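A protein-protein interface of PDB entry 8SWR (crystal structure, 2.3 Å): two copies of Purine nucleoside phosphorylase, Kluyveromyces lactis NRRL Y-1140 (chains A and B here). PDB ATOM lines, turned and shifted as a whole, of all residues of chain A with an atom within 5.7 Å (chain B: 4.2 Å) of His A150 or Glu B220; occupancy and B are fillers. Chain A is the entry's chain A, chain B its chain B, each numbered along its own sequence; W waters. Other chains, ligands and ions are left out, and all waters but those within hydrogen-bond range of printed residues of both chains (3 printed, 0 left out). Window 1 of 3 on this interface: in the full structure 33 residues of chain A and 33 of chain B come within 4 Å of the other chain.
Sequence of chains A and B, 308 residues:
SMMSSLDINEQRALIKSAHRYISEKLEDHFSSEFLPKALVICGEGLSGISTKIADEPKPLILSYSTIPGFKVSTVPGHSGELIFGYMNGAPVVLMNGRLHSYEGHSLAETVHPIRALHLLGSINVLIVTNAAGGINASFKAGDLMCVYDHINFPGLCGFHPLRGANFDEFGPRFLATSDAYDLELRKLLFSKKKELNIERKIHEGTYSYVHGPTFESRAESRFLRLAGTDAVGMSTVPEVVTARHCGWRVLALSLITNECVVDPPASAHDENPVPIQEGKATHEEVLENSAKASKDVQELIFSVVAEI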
ATOM      1  N   VAL A 147       1.929  20.070  28.005  1.00  0.00           N
ATOM      2  CA  VAL A 147       1.397  20.054  26.648  1.00  0.00           C
ATOM      3  C   VAL A 147       0.713  18.719  26.398  1.00  0.00           C
ATOM      4  O   VAL A 147       1.320  17.656  26.574  1.00  0.00           O
ATOM      5  CB  VAL A 147       2.516  20.296  25.624  1.00  0.00           C
ATOM      6  CG1 VAL A 147       1.936  20.444  24.230  1.00  0.00           C
ATOM      7  CG2 VAL A 147       3.347  21.510  26.008  1.00  0.00           C
ATOM      8  N   TYR A 148      -0.554  18.766  25.984  1.00  0.00           N
ATOM      9  CA  TYR A 148      -1.257  17.564  25.560  1.00  0.00           C
ATOM     10  C   TYR A 148      -1.770  17.650  24.127  1.00  0.00           C
ATOM     11  O   TYR A 148      -2.404  16.701  23.650  1.00  0.00           O
ATOM     12  CB  TYR A 148      -2.398  17.226  26.543  1.00  0.00           C
ATOM     13  CG  TYR A 148      -3.667  18.076  26.526  1.00  0.00           C
ATOM     14  CD1 TYR A 148      -3.768  19.249  25.786  1.00  0.00           C
ATOM     15  CD2 TYR A 148      -4.774  17.683  27.274  1.00  0.00           C
ATOM     16  CE1 TYR A 148      -4.938  19.998  25.786  1.00  0.00           C
ATOM     17  CE2 TYR A 148      -5.942  18.424  27.280  1.00  0.00           C
ATOM     18  CZ  TYR A 148      -6.020  19.580  26.537  1.00  0.00           C
ATOM     19  OH  TYR A 148      -7.183  20.318  26.546  1.00  0.00           O
ATOM     20  N   ASP A 149      -1.500  18.751  23.430  1.00  0.00           N
ATOM     21  CA  ASP A 149      -1.829  18.921  22.022  1.00  0.00           C
ATOM     22  C   ASP A 149      -1.036  20.111  21.503  1.00  0.00           C
ATOM     23  O   ASP A 149      -0.559  20.940  22.282  1.00  0.00           O
ATOM     24  CB  ASP A 149      -3.331  19.137  21.809  1.00  0.00           C
ATOM     25  CG  ASP A 149      -3.753  18.910  20.372  1.00  0.00           C
ATOM     26  OD1 ASP A 149      -2.924  18.419  19.578  1.00  0.00           O
ATOM     27  OD2 ASP A 149      -4.913  19.227  20.036  1.00  0.00           O
ATOM     28  N   HIS A 150      -0.893  20.192  20.183  1.00  0.00           N
ATOM     29  CA  HIS A 150      -0.198  21.328  19.598  1.00  0.00           C
ATOM     30  C   HIS A 150      -0.872  21.753  18.301  1.00  0.00           C
ATOM     31  O   HIS A 150      -1.686  21.029  17.723  1.00  0.00           O
ATOM     32  CB  HIS A 150       1.298  21.034  19.364  1.00  0.00           C
ATOM     33  CG  HIS A 150       1.575  19.985  18.329  1.00  0.00           C
ATOM     34  ND1 HIS A 150       2.455  18.947  18.548  1.00  0.00           N
ATOM     35  CD2 HIS A 150       1.122  19.831  17.061  1.00  0.00           C
ATOM     36  CE1 HIS A 150       2.515  18.187  17.469  1.00  0.00           C
ATOM     37  NE2 HIS A 150       1.716  18.702  16.552  1.00  0.00           N
ATOM     38  N   ILE A 151      -0.516  22.956  17.857  1.00  0.00           N
ATOM     39  CA  ILE A 151      -0.867  23.463  16.537  1.00  0.00           C
ATOM     40  C   ILE A 151       0.430  23.746  15.799  1.00  0.00           C
ATOM     41  O   ILE A 151       1.215  24.603  16.222  1.00  0.00           O
ATOM     42  CB  ILE A 151      -1.733  24.729  16.609  1.00  0.00           C
ATOM     43  CG1 ILE A 151      -3.024  24.454  17.371  1.00  0.00           C
ATOM     44  CG2 ILE A 151      -2.033  25.245  15.211  1.00  0.00           C
ATOM     45  CD1 ILE A 151      -3.831  25.690  17.649  1.00  0.00           C
ATOM     46  N   ASN A 152       0.660  23.029  14.704  1.00  0.00           N
ATOM     47  CA  ASN A 152       1.846  23.248  13.879  1.00  0.00           C
ATOM     48  C   ASN A 152       1.446  23.995  12.609  1.00  0.00           C
ATOM     49  O   ASN A 152       1.414  23.449  11.503  1.00  0.00           O
ATOM     50  CB  ASN A 152       2.529  21.922  13.569  1.00  0.00           C
ATOM     51  CG  ASN A 152       3.867  22.099  12.873  1.00  0.00           C
ATOM     52  OD1 ASN A 152       4.354  23.218  12.706  1.00  0.00           O
ATOM     53  ND2 ASN A 152       4.471  20.988  12.464  1.00  0.00           N
ATOM     54  N   PHE A 153       1.117  25.270  12.802  1.00  0.00           N
ATOM     55  CA  PHE A 153       0.722  26.114  11.677  1.00  0.00           C
ATOM     56  C   PHE A 153       1.801  26.235  10.606  1.00  0.00           C
ATOM     57  O   PHE A 153       1.453  26.140   9.417  1.00  0.00           O
ATOM     58  CB  PHE A 153       0.297  27.498  12.180  1.00  0.00           C
ATOM     59  CG  PHE A 153      -0.376  28.338  11.131  1.00  0.00           C
ATOM     60  CD1 PHE A 153      -1.707  28.132  10.812  1.00  0.00           C
ATOM     61  CD2 PHE A 153       0.322  29.334  10.462  1.00  0.00           C
ATOM     62  CE1 PHE A 153      -2.334  28.895   9.843  1.00  0.00           C
ATOM     63  CE2 PHE A 153      -0.299  30.107   9.491  1.00  0.00           C
ATOM     64  CZ  PHE A 153      -1.630  29.886   9.182  1.00  0.00           C
ATOM     65  N   LEU A 156       1.546  23.158   8.495  1.00  0.00           N
ATOM     66  CA  LEU A 156       0.424  23.216   7.563  1.00  0.00           C
ATOM     67  C   LEU A 156       0.772  24.021   6.319  1.00  0.00           C
ATOM     68  O   LEU A 156       0.224  23.767   5.240  1.00  0.00           O
ATOM     69  CB  LEU A 156      -0.802  23.821   8.249  1.00  0.00           C
ATOM     70  CG  LEU A 156      -1.343  23.134   9.506  1.00  0.00           C
ATOM     71  CD1 LEU A 156      -2.607  23.828   9.991  1.00  0.00           C
ATOM     72  CD2 LEU A 156      -1.615  21.663   9.239  1.00  0.00           C
ATOM     73  N   THR A 177      -0.772  12.767  14.459  1.00  0.00           N
ATOM     74  CA  THR A 177      -0.355  13.586  15.587  1.00  0.00           C
ATOM     75  C   THR A 177      -1.455  13.773  16.619  1.00  0.00           C
ATOM     76  O   THR A 177      -1.236  14.475  17.612  1.00  0.00           O
ATOM     77  CB  THR A 177       0.139  14.962  15.109  1.00  0.00           C
ATOM     78  OG1 THR A 177      -0.896  15.617  14.365  1.00  0.00           O
ATOM     79  CG2 THR A 177       1.383  14.819  14.239  1.00  0.00           C
ATOM     80  N   ALA A 180      -0.031  12.484  19.994  1.00  0.00           N
ATOM     81  CA  ALA A 180       1.367  12.872  20.118  1.00  0.00           C
ATOM     82  C   ALA A 180       1.836  12.891  21.567  1.00  0.00           C
ATOM     83  O   ALA A 180       3.005  12.594  21.839  1.00  0.00           O
ATOM     84  CB  ALA A 180       1.586  14.240  19.471  1.00  0.00           C
ATOM     85  N   TYR A 181       0.955  13.222  22.505  1.00  0.00           N
ATOM     86  CA  TYR A 181       1.344  13.488  23.887  1.00  0.00           C
ATOM     87  C   TYR A 181       0.815  12.375  24.785  1.00  0.00           C
ATOM     88  O   TYR A 181      -0.365  12.357  25.148  1.00  0.00           O
ATOM     89  CB  TYR A 181       0.864  14.874  24.298  1.00  0.00           C
ATOM     90  CG  TYR A 181       1.544  15.928  23.454  1.00  0.00           C
ATOM     91  CD1 TYR A 181       2.801  16.411  23.795  1.00  0.00           C
ATOM     92  CD2 TYR A 181       0.953  16.403  22.288  1.00  0.00           C
ATOM     93  CE1 TYR A 181       3.442  17.358  23.012  1.00  0.00           C
ATOM     94  CE2 TYR A 181       1.585  17.350  21.501  1.00  0.00           C
ATOM     95  CZ  TYR A 181       2.827  17.824  21.866  1.00  0.00           C
ATOM     96  OH  TYR A 181       3.451  18.765  21.080  1.00  0.00           O
ATOM     97  N   THR A 206      -2.828  23.484  24.820  1.00  0.00           N
ATOM     98  CA  THR A 206      -2.325  23.359  23.460  1.00  0.00           C
ATOM     99  C   THR A 206      -1.207  24.372  23.236  1.00  0.00           C
ATOM    100  O   THR A 206      -1.399  25.575  23.449  1.00  0.00           O
ATOM    101  CB  THR A 206      -3.451  23.575  22.447  1.00  0.00           C
ATOM    102  OG1 THR A 206      -4.378  22.484  22.524  1.00  0.00           O
ATOM    103  CG2 THR A 206      -2.892  23.661  21.038  1.00  0.00           C
ATOM    104  N   TYR A 207      -0.054  23.881  22.797  1.00  0.00           N
ATOM    105  CA  TYR A 207       1.103  24.707  22.483  1.00  0.00           C
ATOM    106  C   TYR A 207       1.145  24.957  20.981  1.00  0.00           C
ATOM    107  O   TYR A 207       0.880  24.052  20.188  1.00  0.00           O
ATOM    108  CB  TYR A 207       2.387  24.015  22.958  1.00  0.00           C
ATOM    109  CG  TYR A 207       3.691  24.661  22.529  1.00  0.00           C
ATOM    110  CD1 TYR A 207       4.267  24.365  21.298  1.00  0.00           C
ATOM    111  CD2 TYR A 207       4.361  25.546  23.368  1.00  0.00           C
ATOM    112  CE1 TYR A 207       5.460  24.944  20.907  1.00  0.00           C
ATOM    113  CE2 TYR A 207       5.558  26.131  22.983  1.00  0.00           C
ATOM    114  CZ  TYR A 207       6.102  25.825  21.750  1.00  0.00           C
ATOM    115  OH  TYR A 207       7.289  26.392  21.351  1.00  0.00           O
ATOM    116  N   SER A 208       1.469  26.184  20.588  1.00  0.00           N
ATOM    117  CA  SER A 208       1.524  26.552  19.180  1.00  0.00           C
ATOM    118  C   SER A 208       2.939  26.965  18.814  1.00  0.00           C
ATOM    119  O   SER A 208       3.530  27.826  19.472  1.00  0.00           O
ATOM    120  CB  SER A 208       0.549  27.685  18.860  1.00  0.00           C
ATOM    121  OG  SER A 208      -0.748  27.181  18.599  1.00  0.00           O
ATOM    122  N   VAL A 237       7.647  21.701  18.815  1.00  0.00           N
ATOM    123  CA  VAL A 237       6.824  20.885  17.916  1.00  0.00           C
ATOM    124  C   VAL A 237       7.647  20.122  16.878  1.00  0.00           C
ATOM    125  O   VAL A 237       7.411  18.917  16.707  1.00  0.00           O
ATOM    126  CB  VAL A 237       5.716  21.743  17.285  1.00  0.00           C
ATOM    127  CG1 VAL A 237       4.897  20.917  16.300  1.00  0.00           C
ATOM    128  CG2 VAL A 237       4.813  22.313  18.367  1.00  0.00           C
ATOM    129  N   VAL A 240       9.071  17.244  18.686  1.00  0.00           N
ATOM    130  CA  VAL A 240       8.029  16.300  19.083  1.00  0.00           C
ATOM    131  C   VAL A 240       7.606  15.450  17.892  1.00  0.00           C
ATOM    132  O   VAL A 240       7.493  14.222  17.991  1.00  0.00           O
ATOM    133  CB  VAL A 240       6.832  17.050  19.698  1.00  0.00           C
ATOM    134  CG1 VAL A 240       5.611  16.141  19.780  1.00  0.00           C
ATOM    135  CG2 VAL A 240       7.192  17.599  21.071  1.00  0.00           C
ATOM    136  N   VAL A 241       7.371  16.094  16.744  1.00  0.00           N
ATOM    137  CA  VAL A 241       6.986  15.364  15.536  1.00  0.00           C
ATOM    138  C   VAL A 241       8.066  14.358  15.161  1.00  0.00           C
ATOM    139  O   VAL A 241       7.778  13.196  14.851  1.00  0.00           O
ATOM    140  CB  VAL A 241       6.701  16.348  14.384  1.00  0.00           C
ATOM    141  CG1 VAL A 241       6.533  15.602  13.069  1.00  0.00           C
ATOM    142  CG2 VAL A 241       5.466  17.179  14.687  1.00  0.00           C
ATOM    143  N   GLU B 216      -3.631  15.635  10.946  1.00  0.00           N
ATOM    144  CA  GLU B 216      -3.837  16.802  11.788  1.00  0.00           C
ATOM    145  C   GLU B 216      -3.972  16.408  13.252  1.00  0.00           C
ATOM    146  O   GLU B 216      -4.623  15.416  13.591  1.00  0.00           O
ATOM    147  CB  GLU B 216      -5.080  17.569  11.348  1.00  0.00           C
ATOM    148  CG  GLU B 216      -4.907  18.354  10.066  1.00  0.00           C
ATOM    149  CD  GLU B 216      -4.872  17.461   8.849  1.00  0.00           C
ATOM    150  OE1 GLU B 216      -5.473  16.366   8.899  1.00  0.00           O
ATOM    151  OE2 GLU B 216      -4.238  17.847   7.846  1.00  0.00           O
ATOM    152  N   SER B 217      -3.350  17.201  14.119  1.00  0.00           N
ATOM    153  CA  SER B 217      -3.639  17.120  15.536  1.00  0.00           C
ATOM    154  C   SER B 217      -5.090  17.527  15.784  1.00  0.00           C
ATOM    155  O   SER B 217      -5.792  18.013  14.893  1.00  0.00           O
ATOM    156  CB  SER B 217      -2.690  18.015  16.331  1.00  0.00           C
ATOM    157  OG  SER B 217      -3.030  19.382  16.171  1.00  0.00           O
ATOM    158  N   ARG B 218      -5.541  17.317  17.019  1.00  0.00           N
ATOM    159  CA  ARG B 218      -6.920  17.648  17.351  1.00  0.00           C
ATOM    160  C   ARG B 218      -7.175  19.143  17.205  1.00  0.00           C
ATOM    161  O   ARG B 218      -8.206  19.555  16.660  1.00  0.00           O
ATOM    162  CB  ARG B 218      -7.240  17.182  18.769  1.00  0.00           C
ATOM    163  CG  ARG B 218      -7.277  15.673  18.932  1.00  0.00           C
ATOM    164  CD  ARG B 218      -6.594  15.246  20.227  1.00  0.00           C
ATOM    165  NE  ARG B 218      -6.428  13.800  20.305  1.00  0.00           N
ATOM    166  CZ  ARG B 218      -7.390  12.953  20.649  1.00  0.00           C
ATOM    167  NH1 ARG B 218      -8.603  13.376  20.964  1.00  0.00           N
ATOM    168  NH2 ARG B 218      -7.129  11.649  20.672  1.00  0.00           N
ATOM    169  N   ALA B 219      -6.238  19.968  17.672  1.00  0.00           N
ATOM    170  CA  ALA B 219      -6.433  21.411  17.614  1.00  0.00           C
ATOM    171  C   ALA B 219      -6.342  21.929  16.184  1.00  0.00           C
ATOM    172  O   ALA B 219      -7.075  22.850  15.807  1.00  0.00           O
ATOM    173  CB  ALA B 219      -5.412  22.112  18.509  1.00  0.00           C
ATOM    174  N   GLU B 220      -5.448  21.354  15.374  1.00  0.00           N
ATOM    175  CA  GLU B 220      -5.340  21.774  13.981  1.00  0.00           C
ATOM    176  C   GLU B 220      -6.646  21.537  13.234  1.00  0.00           C
ATOM    177  O   GLU B 220      -7.089  22.389  12.454  1.00  0.00           O
ATOM    178  CB  GLU B 220      -4.190  21.037  13.291  1.00  0.00           C
ATOM    179  CG  GLU B 220      -2.802  21.470  13.738  1.00  0.00           C
ATOM    180  CD  GLU B 220      -1.738  20.428  13.435  1.00  0.00           C
ATOM    181  OE1 GLU B 220      -2.080  19.369  12.867  1.00  0.00           O
ATOM    182  OE2 GLU B 220      -0.556  20.667  13.763  1.00  0.00           O
ATOM    183  N   SER B 221      -7.282  20.385  13.467  1.00  0.00           N
ATOM    184  CA  SER B 221      -8.555  20.094  12.816  1.00  0.00           C
ATOM    185  C   SER B 221      -9.640  21.054  13.282  1.00  0.00           C
ATOM    186  O   SER B 221     -10.396  21.595  12.468  1.00  0.00           O
ATOM    187  CB  SER B 221      -8.966  18.648  13.088  1.00  0.00           C
ATOM    188  OG  SER B 221      -8.040  17.742  12.522  1.00  0.00           O
ATOM    189  N   ARG B 222      -9.738  21.269  14.597  1.00  0.00           N
ATOM    190  CA  ARG B 222     -10.688  22.246  15.116  1.00  0.00           C
ATOM    191  C   ARG B 222     -10.425  23.622  14.520  1.00  0.00           C
ATOM    192  O   ARG B 222     -11.365  24.365  14.213  1.00  0.00           O
ATOM    193  CB  ARG B 222     -10.613  22.299  16.644  1.00  0.00           C
ATOM    194  CG  ARG B 222     -11.337  21.157  17.345  1.00  0.00           C
ATOM    195  CD  ARG B 222     -11.522  21.421  18.838  1.00  0.00           C
ATOM    196  NE  ARG B 222     -10.372  22.074  19.453  1.00  0.00           N
ATOM    197  CZ  ARG B 222      -9.368  21.430  20.032  1.00  0.00           C
ATOM    198  NH1 ARG B 222      -9.319  20.107  20.059  1.00  0.00           N
ATOM    199  NH2 ARG B 222      -8.389  22.129  20.601  1.00  0.00           N
ATOM    200  N   PHE B 223      -9.150  23.974  14.340  1.00  0.00           N
ATOM    201  CA  PHE B 223      -8.814  25.233  13.687  1.00  0.00           C
ATOM    202  C   PHE B 223      -9.277  25.235  12.237  1.00  0.00           C
ATOM    203  O   PHE B 223      -9.922  26.187  11.780  1.00  0.00           O
ATOM    204  CB  PHE B 223      -7.309  25.480  13.757  1.00  0.00           C
ATOM    205  CG  PHE B 223      -6.801  26.405  12.689  1.00  0.00           C
ATOM    206  CD1 PHE B 223      -7.182  27.737  12.667  1.00  0.00           C
ATOM    207  CD2 PHE B 223      -5.953  25.938  11.700  1.00  0.00           C
ATOM    208  CE1 PHE B 223      -6.715  28.589  11.681  1.00  0.00           C
ATOM    209  CE2 PHE B 223      -5.484  26.783  10.713  1.00  0.00           C
ATOM    210  CZ  PHE B 223      -5.865  28.109  10.703  1.00  0.00           C
ATOM    211  N   LEU B 224      -8.936  24.182  11.491  1.00  0.00           N
ATOM    212  CA  LEU B 224      -9.362  24.098  10.100  1.00  0.00           C
ATOM    213  C   LEU B 224     -10.877  24.195   9.991  1.00  0.00           C
ATOM    214  O   LEU B 224     -11.403  24.845   9.080  1.00  0.00           O
ATOM    215  CB  LEU B 224      -8.845  22.803   9.469  1.00  0.00           C
ATOM    216  CG  LEU B 224      -7.343  22.774   9.177  1.00  0.00           C
ATOM    217  CD1 LEU B 224      -6.845  21.356   8.954  1.00  0.00           C
ATOM    218  CD2 LEU B 224      -7.029  23.639   7.978  1.00  0.00           C
HETATM  219  O   HOH W   1      -6.913  19.979  21.723  1.00  0.00           O
HETATM  220  O   HOH W   2       0.741  18.228  13.803  1.00  0.00           O
HETATM  221  O   HOH W   3      -3.389  13.182  13.535  1.00  0.00           O
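OD2 of Asp A149 sits at hydrogen-bond distance from N of Ala B219 (2.8 Å). The backbone carbonyl oxygen of His A150 sits at hydrogen-bond distance from the side-chain hydroxyl of Ser B217, at 2.6 Å. The backbone NH of Asn A152 sits at hydrogen-bond distance from the side-chain carboxylate of Glu B220. OG1 of Thr A177 lies within hydrogen-bond range of N of Ser B217 (2.9 Å).
O of Asp A149 sits at hydrogen-bond distance from N of Tyr A207, 3.0 Å away. ND1 of His A150 lies within hydrogen-bond range of OH of Tyr A181 (2.7 Å). N of Ile A151 is in hydrogen-bond range of O of Tyr A207 (2.9 Å). The backbone NH (N) of Ser B217 sits at hydrogen-bond distance from the side-chain carboxylate (OE1) of Glu B220 (2.8 Å). The backbone carbonyl oxygen (O) of Ser B217 is in hydrogen-bond range of the side-chain hydroxyl (OG) of Ser B221 (3.3 Å).
OD1 of Asp A149 touches CB of Ser B217, at 3.3 Å. Asp A149 touches Arg B218. O of His A150 touches CB of Ala B219, at 3.96 Å. Glu B220 touches His A150 (OE2 to CD2, 3.8 Å). CB of Ala B219 touches CG1 of Ile A151, 3.5 Å away. Ile A151 touches Glu B220. CZ of Phe B223 touches CE1 of Phe A153, at 3.7 Å. Glu B216 touches Thr A177 (C to OG1, 3.4 Å). Thr A206 touches Ala B219 (CG2 to CB, 3.9 Å).
Of chain B, only Ser B217 (2.6 Å), Ala B219 (3.96 Å) and Glu B220 (3.8 Å) come within 4 Å of His A150. Of the printed residues of chain B, Ile A151 touches Ala B219 (3.5 Å) and Glu B220 (3.8 Å). Of the printed residues of chain B, Phe A153 touches Phe B223. Of the printed residues of chain A, Arg B218 touches Asp A149 (3.3 Å). The nearest printed residue of chain B that does not touch His A150 is Arg B218 (5.4 Å). The nearest residue of chain A that does not touch Glu B220 is Thr A177 (4.2 Å).
Of the 17 printed residues of chain A, 7 touch a printed residue of chain B. Printed residues of chain A that touch a printed residue of chain B: Asp A149, His A150, Ile A151, Asn A152, Phe A153, Thr A177 and Thr A206. Hydrophobic or aromatic side chains of chain A within 4 Å of the printed part of chain B: His A150, Ile A151 and Phe A153. Of the 9 printed residues of chain B, 6 touch a printed residue of chain A. Among the printed residues, 13 pairs touch across the chains. Among the printed residues, no Asp or Glu carboxylate lies within 4 Å of a Lys or Arg side-chain nitrogen of the other chain.
No position is printed for both chains. Of the 13 pairs that touch across the chains among the printed residues, none has its exchanged pair printed and touching as well.
Water W3 bridges the backbone carbonyl oxygen (O) of Glu B216 and the backbone NH (N) of Thr A177. Water W1 bridges the side-chain carboxylate of Asp A149 (2.7 Å) and the guanidinium group of Arg B222 (2.8 Å). Water W2 lies within hydrogen-bond range of the side-chain carboxylate of Glu B220 (2.8 Å), a ring nitrogen (NE2) of His A150 (3.0 Å) and the side-chain hydroxyl of Thr A177 (3.1 Å).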
